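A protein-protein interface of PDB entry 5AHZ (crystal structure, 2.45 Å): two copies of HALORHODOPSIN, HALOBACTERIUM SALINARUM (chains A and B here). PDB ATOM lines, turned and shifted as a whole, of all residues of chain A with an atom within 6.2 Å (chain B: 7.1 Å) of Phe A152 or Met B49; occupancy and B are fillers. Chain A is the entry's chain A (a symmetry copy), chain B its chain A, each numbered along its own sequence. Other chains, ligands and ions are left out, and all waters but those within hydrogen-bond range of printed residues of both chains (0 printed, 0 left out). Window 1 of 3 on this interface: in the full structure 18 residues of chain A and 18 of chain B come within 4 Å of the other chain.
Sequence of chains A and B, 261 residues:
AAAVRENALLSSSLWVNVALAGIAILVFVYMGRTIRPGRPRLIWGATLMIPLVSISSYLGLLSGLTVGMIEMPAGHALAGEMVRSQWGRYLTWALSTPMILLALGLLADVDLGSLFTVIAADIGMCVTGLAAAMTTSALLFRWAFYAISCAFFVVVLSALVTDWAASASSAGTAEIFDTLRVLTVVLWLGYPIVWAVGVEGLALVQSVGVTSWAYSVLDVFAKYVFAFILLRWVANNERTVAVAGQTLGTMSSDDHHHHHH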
ATOM      1  N   THR A 117      28.485 -19.602 -20.039  1.00  0.00           N
ATOM      2  CA  THR A 117      28.883 -20.886 -19.460  1.00  0.00           C
ATOM      3  C   THR A 117      29.909 -20.744 -18.329  1.00  0.00           C
ATOM      4  O   THR A 117      29.853 -21.460 -17.316  1.00  0.00           O
ATOM      5  CB  THR A 117      29.466 -21.824 -20.543  1.00  0.00           C
ATOM      6  OG1 THR A 117      28.501 -22.009 -21.587  1.00  0.00           O
ATOM      7  CG2 THR A 117      29.824 -23.171 -19.955  1.00  0.00           C
ATOM      8  N   ALA A 120      28.142 -19.398 -15.416  1.00  0.00           N
ATOM      9  CA  ALA A 120      27.319 -20.462 -14.849  1.00  0.00           C
ATOM     10  C   ALA A 120      28.191 -21.408 -14.016  1.00  0.00           C
ATOM     11  O   ALA A 120      27.811 -21.803 -12.908  1.00  0.00           O
ATOM     12  CB  ALA A 120      26.571 -21.236 -15.947  1.00  0.00           C
ATOM     13  N   ALA A 121      29.362 -21.758 -14.544  1.00  0.00           N
ATOM     14  CA  ALA A 121      30.273 -22.622 -13.806  1.00  0.00           C
ATOM     15  C   ALA A 121      30.712 -21.928 -12.539  1.00  0.00           C
ATOM     16  O   ALA A 121      30.904 -22.566 -11.499  1.00  0.00           O
ATOM     17  CB  ALA A 121      31.478 -22.997 -14.657  1.00  0.00           C
ATOM     18  N   ASP A 122      30.872 -20.615 -12.628  1.00  0.00           N
ATOM     19  CA  ASP A 122      31.333 -19.845 -11.485  1.00  0.00           C
ATOM     20  C   ASP A 122      30.274 -19.804 -10.383  1.00  0.00           C
ATOM     21  O   ASP A 122      30.597 -19.896  -9.196  1.00  0.00           O
ATOM     22  CB  ASP A 122      31.710 -18.430 -11.906  1.00  0.00           C
ATOM     23  CG  ASP A 122      31.997 -17.535 -10.720  1.00  0.00           C
ATOM     24  OD1 ASP A 122      31.043 -16.952 -10.161  1.00  0.00           O
ATOM     25  OD2 ASP A 122      33.173 -17.418 -10.330  1.00  0.00           O
ATOM     26  N   ILE A 123      29.007 -19.673 -10.769  1.00  0.00           N
ATOM     27  CA  ILE A 123      27.949 -19.625  -9.767  1.00  0.00           C
ATOM     28  C   ILE A 123      27.798 -21.009  -9.116  1.00  0.00           C
ATOM     29  O   ILE A 123      27.594 -21.113  -7.904  1.00  0.00           O
ATOM     30  CB  ILE A 123      26.626 -19.114 -10.381  1.00  0.00           C
ATOM     31  CG1 ILE A 123      26.787 -17.638 -10.738  1.00  0.00           C
ATOM     32  CG2 ILE A 123      25.480 -19.265  -9.406  1.00  0.00           C
ATOM     33  CD1 ILE A 123      25.674 -17.066 -11.577  1.00  0.00           C
ATOM     34  N   GLY A 124      27.955 -22.065  -9.908  1.00  0.00           N
ATOM     35  CA  GLY A 124      28.038 -23.422  -9.384  1.00  0.00           C
ATOM     36  C   GLY A 124      29.165 -23.661  -8.375  1.00  0.00           C
ATOM     37  O   GLY A 124      28.962 -24.306  -7.328  1.00  0.00           O
ATOM     38  N   MET A 125      30.354 -23.152  -8.687  1.00  0.00           N
ATOM     39  CA  MET A 125      31.493 -23.205  -7.756  1.00  0.00           C
ATOM     40  C   MET A 125      31.130 -22.587  -6.393  1.00  0.00           C
ATOM     41  O   MET A 125      31.367 -23.187  -5.347  1.00  0.00           O
ATOM     42  CB  MET A 125      32.713 -22.474  -8.356  1.00  0.00           C
ATOM     43  CG  MET A 125      33.976 -22.468  -7.484  1.00  0.00           C
ATOM     44  SD  MET A 125      35.296 -21.451  -8.185  1.00  0.00           S
ATOM     45  CE  MET A 125      34.606 -19.804  -7.893  1.00  0.00           C
ATOM     46  N   CYS A 126      30.538 -21.390  -6.424  1.00  0.00           N
ATOM     47  CA  CYS A 126      30.250 -20.643  -5.214  1.00  0.00           C
ATOM     48  C   CYS A 126      29.167 -21.312  -4.381  1.00  0.00           C
ATOM     49  O   CYS A 126      29.282 -21.401  -3.154  1.00  0.00           O
ATOM     50  CB  CYS A 126      29.844 -19.204  -5.559  1.00  0.00           C
ATOM     51  SG  CYS A 126      31.209 -18.220  -6.209  1.00  0.00           S
ATOM     52  N   THR A 128      28.133 -24.533  -4.433  1.00  0.00           N
ATOM     53  CA  THR A 128      28.522 -25.821  -3.861  1.00  0.00           C
ATOM     54  C   THR A 128      29.544 -25.608  -2.726  1.00  0.00           C
ATOM     55  O   THR A 128      29.601 -26.403  -1.791  1.00  0.00           O
ATOM     56  CB  THR A 128      29.049 -26.809  -4.939  1.00  0.00           C
ATOM     57  OG1 THR A 128      30.106 -26.217  -5.705  1.00  0.00           O
ATOM     58  CG2 THR A 128      27.903 -27.192  -5.884  1.00  0.00           C
ATOM     59  N   ALA A 147      34.768 -31.065  -3.598  1.00  0.00           N
ATOM     60  CA  ALA A 147      35.344 -31.596  -4.837  1.00  0.00           C
ATOM     61  C   ALA A 147      34.552 -31.180  -6.086  1.00  0.00           C
ATOM     62  O   ALA A 147      35.147 -30.843  -7.130  1.00  0.00           O
ATOM     63  CB  ALA A 147      35.455 -33.109  -4.755  1.00  0.00           C
ATOM     64  N   ILE A 148      33.222 -31.209  -5.981  1.00  0.00           N
ATOM     65  CA  ILE A 148      32.342 -30.702  -7.040  1.00  0.00           C
ATOM     66  C   ILE A 148      32.640 -29.225  -7.343  1.00  0.00           C
ATOM     67  O   ILE A 148      32.739 -28.808  -8.504  1.00  0.00           O
ATOM     68  CB  ILE A 148      30.851 -30.820  -6.664  1.00  0.00           C
ATOM     69  CG1 ILE A 148      30.495 -32.263  -6.334  1.00  0.00           C
ATOM     70  CG2 ILE A 148      29.978 -30.332  -7.810  1.00  0.00           C
ATOM     71  CD1 ILE A 148      30.870 -33.213  -7.436  1.00  0.00           C
ATOM     72  N   SER A 149      32.746 -28.443  -6.276  1.00  0.00           N
ATOM     73  CA  SER A 149      33.138 -27.046  -6.366  1.00  0.00           C
ATOM     74  C   SER A 149      34.467 -26.860  -7.115  1.00  0.00           C
ATOM     75  O   SER A 149      34.557 -26.014  -8.007  1.00  0.00           O
ATOM     76  CB  SER A 149      33.227 -26.443  -4.966  1.00  0.00           C
ATOM     77  OG  SER A 149      33.449 -25.059  -5.049  1.00  0.00           O
ATOM     78  N   CYS A 150      35.486 -27.653  -6.766  1.00  0.00           N
ATOM     79  CA  CYS A 150      36.739 -27.659  -7.537  1.00  0.00           C
ATOM     80  C   CYS A 150      36.531 -27.958  -9.043  1.00  0.00           C
ATOM     81  O   CYS A 150      37.171 -27.332  -9.895  1.00  0.00           O
ATOM     82  CB  CYS A 150      37.732 -28.678  -6.949  1.00  0.00           C
ATOM     83  SG  CYS A 150      38.438 -28.312  -5.297  1.00  0.00           S
ATOM     84  N   ALA A 151      35.655 -28.914  -9.373  1.00  0.00           N
ATOM     85  CA  ALA A 151      35.347 -29.228 -10.778  1.00  0.00           C
ATOM     86  C   ALA A 151      34.821 -28.000 -11.526  1.00  0.00           C
ATOM     87  O   ALA A 151      35.207 -27.756 -12.675  1.00  0.00           O
ATOM     88  CB  ALA A 151      34.330 -30.379 -10.872  1.00  0.00           C
ATOM     89  N   PHE A 152      33.942 -27.236 -10.869  1.00  0.00           N
ATOM     90  CA  PHE A 152      33.436 -25.988 -11.431  1.00  0.00           C
ATOM     91  C   PHE A 152      34.565 -24.992 -11.645  1.00  0.00           C
ATOM     92  O   PHE A 152      34.656 -24.379 -12.697  1.00  0.00           O
ATOM     93  CB  PHE A 152      32.369 -25.361 -10.521  1.00  0.00           C
ATOM     94  CG  PHE A 152      30.996 -25.915 -10.732  1.00  0.00           C
ATOM     95  CD1 PHE A 152      30.382 -25.829 -11.979  1.00  0.00           C
ATOM     96  CD2 PHE A 152      30.307 -26.511  -9.689  1.00  0.00           C
ATOM     97  CE1 PHE A 152      29.120 -26.342 -12.174  1.00  0.00           C
ATOM     98  CE2 PHE A 152      29.034 -27.026  -9.886  1.00  0.00           C
ATOM     99  CZ  PHE A 152      28.439 -26.941 -11.126  1.00  0.00           C
ATOM    100  N   PHE A 153      35.397 -24.818 -10.621  1.00  0.00           N
ATOM    101  CA  PHE A 153      36.556 -23.925 -10.677  1.00  0.00           C
ATOM    102  C   PHE A 153      37.432 -24.228 -11.909  1.00  0.00           C
ATOM    103  O   PHE A 153      37.853 -23.329 -12.639  1.00  0.00           O
ATOM    104  CB  PHE A 153      37.367 -24.066  -9.375  1.00  0.00           C
ATOM    105  CG  PHE A 153      38.485 -23.063  -9.222  1.00  0.00           C
ATOM    106  CD1 PHE A 153      38.498 -21.883  -9.949  1.00  0.00           C
ATOM    107  CD2 PHE A 153      39.540 -23.312  -8.339  1.00  0.00           C
ATOM    108  CE1 PHE A 153      39.531 -20.971  -9.792  1.00  0.00           C
ATOM    109  CE2 PHE A 153      40.577 -22.399  -8.180  1.00  0.00           C
ATOM    110  CZ  PHE A 153      40.578 -21.235  -8.913  1.00  0.00           C
ATOM    111  N   VAL A 154      37.679 -25.508 -12.136  1.00  0.00           N
ATOM    112  CA  VAL A 154      38.450 -25.971 -13.281  1.00  0.00           C
ATOM    113  C   VAL A 154      37.833 -25.550 -14.610  1.00  0.00           C
ATOM    114  O   VAL A 154      38.535 -25.095 -15.507  1.00  0.00           O
ATOM    115  CB  VAL A 154      38.590 -27.496 -13.234  1.00  0.00           C
ATOM    116  CG1 VAL A 154      38.883 -28.061 -14.610  1.00  0.00           C
ATOM    117  CG2 VAL A 154      39.653 -27.893 -12.201  1.00  0.00           C
ATOM    118  N   VAL A 155      36.514 -25.688 -14.728  1.00  0.00           N
ATOM    119  CA  VAL A 155      35.794 -25.175 -15.891  1.00  0.00           C
ATOM    120  C   VAL A 155      36.078 -23.701 -16.113  1.00  0.00           C
ATOM    121  O   VAL A 155      36.372 -23.280 -17.229  1.00  0.00           O
ATOM    122  CB  VAL A 155      34.275 -25.350 -15.755  1.00  0.00           C
ATOM    123  CG1 VAL A 155      33.576 -24.700 -16.929  1.00  0.00           C
ATOM    124  CG2 VAL A 155      33.922 -26.812 -15.654  1.00  0.00           C
ATOM    125  N   VAL A 156      35.982 -22.914 -15.044  1.00  0.00           N
ATOM    126  CA  VAL A 156      36.270 -21.484 -15.118  1.00  0.00           C
ATOM    127  C   VAL A 156      37.726 -21.238 -15.529  1.00  0.00           C
ATOM    128  O   VAL A 156      38.002 -20.446 -16.433  1.00  0.00           O
ATOM    129  CB  VAL A 156      35.964 -20.797 -13.778  1.00  0.00           C
ATOM    130  CG1 VAL A 156      36.657 -19.452 -13.687  1.00  0.00           C
ATOM    131  CG2 VAL A 156      34.434 -20.671 -13.592  1.00  0.00           C
ATOM    132  N   LEU A 157      38.647 -21.954 -14.890  1.00  0.00           N
ATOM    133  CA  LEU A 157      40.084 -21.815 -15.172  1.00  0.00           C
ATOM    134  C   LEU A 157      40.468 -22.144 -16.627  1.00  0.00           C
ATOM    135  O   LEU A 157      41.240 -21.408 -17.250  1.00  0.00           O
ATOM    136  CB  LEU A 157      40.885 -22.707 -14.219  1.00  0.00           C
ATOM    137  CG  LEU A 157      40.903 -22.306 -12.743  1.00  0.00           C
ATOM    138  CD1 LEU A 157      41.431 -23.444 -11.853  1.00  0.00           C
ATOM    139  CD2 LEU A 157      41.733 -21.041 -12.549  1.00  0.00           C
ATOM    140  N   ILE B  25      29.627 -37.253 -16.458  1.00  0.00           N
ATOM    141  CA  ILE B  25      30.636 -36.198 -16.455  1.00  0.00           C
ATOM    142  C   ILE B  25      31.941 -36.744 -17.049  1.00  0.00           C
ATOM    143  O   ILE B  25      32.496 -36.165 -17.988  1.00  0.00           O
ATOM    144  CB  ILE B  25      30.878 -35.642 -15.039  1.00  0.00           C
ATOM    145  CG1 ILE B  25      29.695 -34.785 -14.583  1.00  0.00           C
ATOM    146  CG2 ILE B  25      32.149 -34.835 -14.992  1.00  0.00           C
ATOM    147  CD1 ILE B  25      29.505 -34.743 -13.038  1.00  0.00           C
ATOM    148  N   PHE B  28      31.475 -37.346 -20.820  1.00  0.00           N
ATOM    149  CA  PHE B  28      31.350 -36.096 -21.577  1.00  0.00           C
ATOM    150  C   PHE B  28      32.703 -35.396 -21.684  1.00  0.00           C
ATOM    151  O   PHE B  28      33.030 -34.820 -22.717  1.00  0.00           O
ATOM    152  CB  PHE B  28      30.305 -35.165 -20.950  1.00  0.00           C
ATOM    153  CG  PHE B  28      28.889 -35.717 -20.994  1.00  0.00           C
ATOM    154  CD1 PHE B  28      28.596 -36.876 -21.716  1.00  0.00           C
ATOM    155  CD2 PHE B  28      27.854 -35.076 -20.314  1.00  0.00           C
ATOM    156  CE1 PHE B  28      27.313 -37.376 -21.759  1.00  0.00           C
ATOM    157  CE2 PHE B  28      26.567 -35.577 -20.339  1.00  0.00           C
ATOM    158  CZ  PHE B  28      26.287 -36.732 -21.064  1.00  0.00           C
ATOM    159  N   TRP B  44      29.475 -27.954 -26.036  1.00  0.00           N
ATOM    160  CA  TRP B  44      30.009 -28.977 -25.150  1.00  0.00           C
ATOM    161  C   TRP B  44      30.198 -28.480 -23.724  1.00  0.00           C
ATOM    162  O   TRP B  44      29.880 -29.191 -22.774  1.00  0.00           O
ATOM    163  CB  TRP B  44      31.331 -29.487 -25.711  1.00  0.00           C
ATOM    164  CG  TRP B  44      32.188 -30.245 -24.753  1.00  0.00           C
ATOM    165  CD1 TRP B  44      32.066 -31.555 -24.408  1.00  0.00           C
ATOM    166  CD2 TRP B  44      33.338 -29.752 -24.052  1.00  0.00           C
ATOM    167  NE1 TRP B  44      33.058 -31.906 -23.520  1.00  0.00           N
ATOM    168  CE2 TRP B  44      33.852 -30.818 -23.288  1.00  0.00           C
ATOM    169  CE3 TRP B  44      33.976 -28.507 -23.987  1.00  0.00           C
ATOM    170  CZ2 TRP B  44      34.969 -30.681 -22.469  1.00  0.00           C
ATOM    171  CZ3 TRP B  44      35.086 -28.373 -23.177  1.00  0.00           C
ATOM    172  CH2 TRP B  44      35.574 -29.452 -22.429  1.00  0.00           C
ATOM    173  N   GLY B  45      30.716 -27.260 -23.576  1.00  0.00           N
ATOM    174  CA  GLY B  45      30.909 -26.670 -22.258  1.00  0.00           C
ATOM    175  C   GLY B  45      29.598 -26.492 -21.512  1.00  0.00           C
ATOM    176  O   GLY B  45      29.448 -26.882 -20.353  1.00  0.00           O
ATOM    177  N   ALA B  46      28.637 -25.897 -22.195  1.00  0.00           N
ATOM    178  CA  ALA B  46      27.283 -25.785 -21.695  1.00  0.00           C
ATOM    179  C   ALA B  46      26.677 -27.163 -21.319  1.00  0.00           C
ATOM    180  O   ALA B  46      25.968 -27.291 -20.317  1.00  0.00           O
ATOM    181  CB  ALA B  46      26.413 -25.072 -22.741  1.00  0.00           C
ATOM    182  N   THR B  47      26.971 -28.191 -22.110  1.00  0.00           N
ATOM    183  CA  THR B  47      26.357 -29.507 -21.910  1.00  0.00           C
ATOM    184  C   THR B  47      26.920 -30.228 -20.672  1.00  0.00           C
ATOM    185  O   THR B  47      26.193 -30.914 -19.934  1.00  0.00           O
ATOM    186  CB  THR B  47      26.544 -30.385 -23.164  1.00  0.00           C
ATOM    187  OG1 THR B  47      25.828 -29.800 -24.267  1.00  0.00           O
ATOM    188  CG2 THR B  47      26.026 -31.782 -22.927  1.00  0.00           C
ATOM    189  N   LEU B  48      28.216 -30.033 -20.441  1.00  0.00           N
ATOM    190  CA  LEU B  48      28.927 -30.626 -19.314  1.00  0.00           C
ATOM    191  C   LEU B  48      28.453 -30.103 -17.958  1.00  0.00           C
ATOM    192  O   LEU B  48      28.546 -30.804 -16.950  1.00  0.00           O
ATOM    193  CB  LEU B  48      30.409 -30.360 -19.471  1.00  0.00           C
ATOM    194  CG  LEU B  48      31.375 -30.771 -18.379  1.00  0.00           C
ATOM    195  CD1 LEU B  48      31.379 -32.283 -18.246  1.00  0.00           C
ATOM    196  CD2 LEU B  48      32.754 -30.233 -18.758  1.00  0.00           C
ATOM    197  N   MET B  49      27.957 -28.865 -17.944  1.00  0.00           N
ATOM    198  CA  MET B  49      27.435 -28.251 -16.724  1.00  0.00           C
ATOM    199  C   MET B  49      26.235 -29.024 -16.234  1.00  0.00           C
ATOM    200  O   MET B  49      25.996 -29.105 -15.027  1.00  0.00           O
ATOM    201  CB  MET B  49      27.032 -26.796 -16.962  1.00  0.00           C
ATOM    202  CG  MET B  49      28.183 -25.895 -17.309  1.00  0.00           C
ATOM    203  SD  MET B  49      29.113 -25.499 -15.832  1.00  0.00           S
ATOM    204  CE  MET B  49      27.783 -24.837 -14.813  1.00  0.00           C
ATOM    205  N   ILE B  50      25.481 -29.588 -17.178  1.00  0.00           N
ATOM    206  CA  ILE B  50      24.226 -30.245 -16.833  1.00  0.00           C
ATOM    207  C   ILE B  50      24.411 -31.334 -15.758  1.00  0.00           C
ATOM    208  O   ILE B  50      23.774 -31.235 -14.710  1.00  0.00           O
ATOM    209  CB  ILE B  50      23.526 -30.838 -18.059  1.00  0.00           C
ATOM    210  CG1 ILE B  50      23.154 -29.735 -19.049  1.00  0.00           C
ATOM    211  CG2 ILE B  50      22.305 -31.612 -17.618  1.00  0.00           C
ATOM    212  CD1 ILE B  50      22.783 -30.255 -20.428  1.00  0.00           C
ATOM    213  N   PRO B  51      25.302 -32.335 -15.980  1.00  0.00           N
ATOM    214  CA  PRO B  51      25.462 -33.341 -14.915  1.00  0.00           C
ATOM    215  C   PRO B  51      26.224 -32.815 -13.687  1.00  0.00           C
ATOM    216  O   PRO B  51      26.038 -33.326 -12.579  1.00  0.00           O
ATOM    217  CB  PRO B  51      26.265 -34.467 -15.589  1.00  0.00           C
ATOM    218  CG  PRO B  51      26.320 -34.134 -17.019  1.00  0.00           C
ATOM    219  CD  PRO B  51      26.126 -32.663 -17.158  1.00  0.00           C
ATOM    220  N   LEU B  52      27.079 -31.817 -13.880  1.00  0.00           N
ATOM    221  CA  LEU B  52      27.752 -31.207 -12.733  1.00  0.00           C
ATOM    222  C   LEU B  52      26.752 -30.609 -11.743  1.00  0.00           C
ATOM    223  O   LEU B  52      26.951 -30.714 -10.540  1.00  0.00           O
ATOM    224  CB  LEU B  52      28.733 -30.133 -13.188  1.00  0.00           C
ATOM    225  CG  LEU B  52      30.126 -30.670 -13.506  1.00  0.00           C
ATOM    226  CD1 LEU B  52      31.070 -29.549 -13.992  1.00  0.00           C
ATOM    227  CD2 LEU B  52      30.678 -31.373 -12.283  1.00  0.00           C
ATOM    228  N   VAL B  53      25.689 -29.980 -12.249  1.00  0.00           N
ATOM    229  CA  VAL B  53      24.623 -29.458 -11.390  1.00  0.00           C
ATOM    230  C   VAL B  53      23.805 -30.602 -10.775  1.00  0.00           C
ATOM    231  O   VAL B  53      23.467 -30.601  -9.576  1.00  0.00           O
ATOM    232  CB  VAL B  53      23.652 -28.513 -12.165  1.00  0.00           C
ATOM    233  CG1 VAL B  53      22.587 -27.964 -11.229  1.00  0.00           C
ATOM    234  CG2 VAL B  53      24.409 -27.379 -12.852  1.00  0.00           C
ATOM    235  N   SER B  54      23.481 -31.578 -11.614  1.00  0.00           N
ATOM    236  CA  SER B  54      22.691 -32.717 -11.170  1.00  0.00           C
ATOM    237  C   SER B  54      23.377 -33.477 -10.027  1.00  0.00           C
ATOM    238  O   SER B  54      22.716 -33.852  -9.043  1.00  0.00           O
ATOM    239  CB  SER B  54      22.413 -33.659 -12.341  1.00  0.00           C
ATOM    240  OG  SER B  54      21.671 -34.772 -11.901  1.00  0.00           O
ATOM    241  N   ILE B  55      24.689 -33.698 -10.125  1.00  0.00           N
ATOM    242  CA  ILE B  55      25.335 -34.457  -9.052  1.00  0.00           C
ATOM    243  C   ILE B  55      25.326 -33.609  -7.767  1.00  0.00           C
ATOM    244  O   ILE B  55      25.147 -34.144  -6.664  1.00  0.00           O
ATOM    245  CB  ILE B  55      26.788 -34.943  -9.434  1.00  0.00           C
ATOM    246  CG1 ILE B  55      27.227 -36.097  -8.533  1.00  0.00           C
ATOM    247  CG2 ILE B  55      27.804 -33.839  -9.387  1.00  0.00           C
ATOM    248  CD1 ILE B  55      28.526 -36.797  -9.005  1.00  0.00           C
ATOM    249  N   SER B  56      25.464 -32.291  -7.916  1.00  0.00           N
ATOM    250  CA  SER B  56      25.396 -31.374  -6.767  1.00  0.00           C
ATOM    251  C   SER B  56      24.043 -31.459  -6.085  1.00  0.00           C
ATOM    252  O   SER B  56      23.940 -31.602  -4.855  1.00  0.00           O
ATOM    253  CB  SER B  56      25.645 -29.935  -7.207  1.00  0.00           C
ATOM    254  OG  SER B  56      26.860 -29.851  -7.907  1.00  0.00           O
ATOM    255  N   LEU B  95      18.925 -23.920 -11.841  1.00  0.00           N
ATOM    256  CA  LEU B  95      20.244 -23.719 -12.429  1.00  0.00           C
ATOM    257  C   LEU B  95      20.521 -24.756 -13.528  1.00  0.00           C
ATOM    258  O   LEU B  95      21.210 -24.462 -14.503  1.00  0.00           O
ATOM    259  CB  LEU B  95      21.340 -23.776 -11.360  1.00  0.00           C
ATOM    260  CG  LEU B  95      22.751 -23.660 -11.958  1.00  0.00           C
ATOM    261  CD1 LEU B  95      22.946 -22.292 -12.610  1.00  0.00           C
ATOM    262  CD2 LEU B  95      23.838 -23.928 -10.940  1.00  0.00           C
ATOM    263  N   SER B  96      19.976 -25.963 -13.386  1.00  0.00           N
ATOM    264  CA  SER B  96      20.254 -27.005 -14.367  1.00  0.00           C
ATOM    265  C   SER B  96      19.398 -26.856 -15.632  1.00  0.00           C
ATOM    266  O   SER B  96      19.930 -27.022 -16.730  1.00  0.00           O
ATOM    267  CB  SER B  96      20.061 -28.402 -13.764  1.00  0.00           C
ATOM    268  OG  SER B  96      18.706 -28.666 -13.462  1.00  0.00           O
ATOM    269  N   MET B  99      20.810 -24.645 -18.058  1.00  0.00           N
ATOM    270  CA  MET B  99      21.945 -25.172 -18.814  1.00  0.00           C
ATOM    271  C   MET B  99      21.449 -25.923 -20.051  1.00  0.00           C
ATOM    272  O   MET B  99      22.048 -25.821 -21.124  1.00  0.00           O
ATOM    273  CB  MET B  99      22.832 -26.074 -17.964  1.00  0.00           C
ATOM    274  CG  MET B  99      23.544 -25.357 -16.838  1.00  0.00           C
ATOM    275  SD  MET B  99      24.254 -23.776 -17.340  1.00  0.00           S
ATOM    276  CE  MET B  99      25.302 -24.241 -18.717  1.00  0.00           C
ATOM    277  N   LEU B 102      20.397 -23.353 -22.600  1.00  0.00           N
ATOM    278  CA  LEU B 102      21.564 -22.735 -23.206  1.00  0.00           C
ATOM    279  C   LEU B 102      22.147 -23.627 -24.311  1.00  0.00           C
ATOM    280  O   LEU B 102      22.445 -23.152 -25.412  1.00  0.00           O
ATOM    281  CB  LEU B 102      22.622 -22.427 -22.149  1.00  0.00           C
ATOM    282  CG  LEU B 102      23.902 -21.802 -22.711  1.00  0.00           C
ATOM    283  CD1 LEU B 102      23.604 -20.555 -23.575  1.00  0.00           C
ATOM    284  CD2 LEU B 102      24.896 -21.505 -21.587  1.00  0.00           C
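The side-chain hydroxyl (OG1) of Thr A128 is in hydrogen-bond range of the backbone carbonyl oxygen (O) of Gly A124 (2.8 Å).
O of Met A125 sits at hydrogen-bond distance from OG1 of Thr A128, at 3.3 Å.
The backbone carbonyl oxygen (O) of Leu B52 sits at hydrogen-bond distance from the side-chain hydroxyl (OG) of Ser B56, at 2.8 Å.
Thr A117 touches Gly B45 (CG2 to C, 3.7 Å).
N of Ala B46 touches CG2 of Thr A117, at 3.7 Å.
OG1 of Thr A117 touches CD2 of Leu B102 (3.6 Å).
Met B99 touches Ala A120.
Ala A121 touches Met B49 (N to CE, 3.5 Å).
Thr A128 touches Ser B56.
CD1 of Ile A148 touches CG2 of Ile B55, at 3.7 Å.
Ser B56 touches Ile A148 (OG to CG2, 3.2 Å).
Phe A152 touches Met B49 (CE1 to CE, 3.3 Å).
CZ of Phe A152 touches CB of Leu B52, 3.8 Å away.
Phe A152 touches just these residues of chain B: Met B49 (3.3 Å) and Leu B52 (3.8 Å).
Printed residues of chain B within 4 Å of Ile A148: Ile B55 and Ser B56.
Printed residues of chain B within 4 Å of Thr A117: Gly B45, Ala B46 and Leu B102.
Printed residues of chain B within 4 Å of Thr A128: Ser B56.
Hydrophobic or aromatic side chains of chain A that line the printed part of chain B: Ala A120, Ala A121, Ile A148 and Phe A152.
Hydrophobic or aromatic side chains of chain B within 4 Å of the printed part of chain A: Ala B46, Met B49, Leu B52, Ile B55, Met B99 and Leu B102.
Among the printed residues, no Asp or Glu carboxylate lies within 4 Å of a Lys or Arg side-chain nitrogen of the other chain.
No position is printed for both chains.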
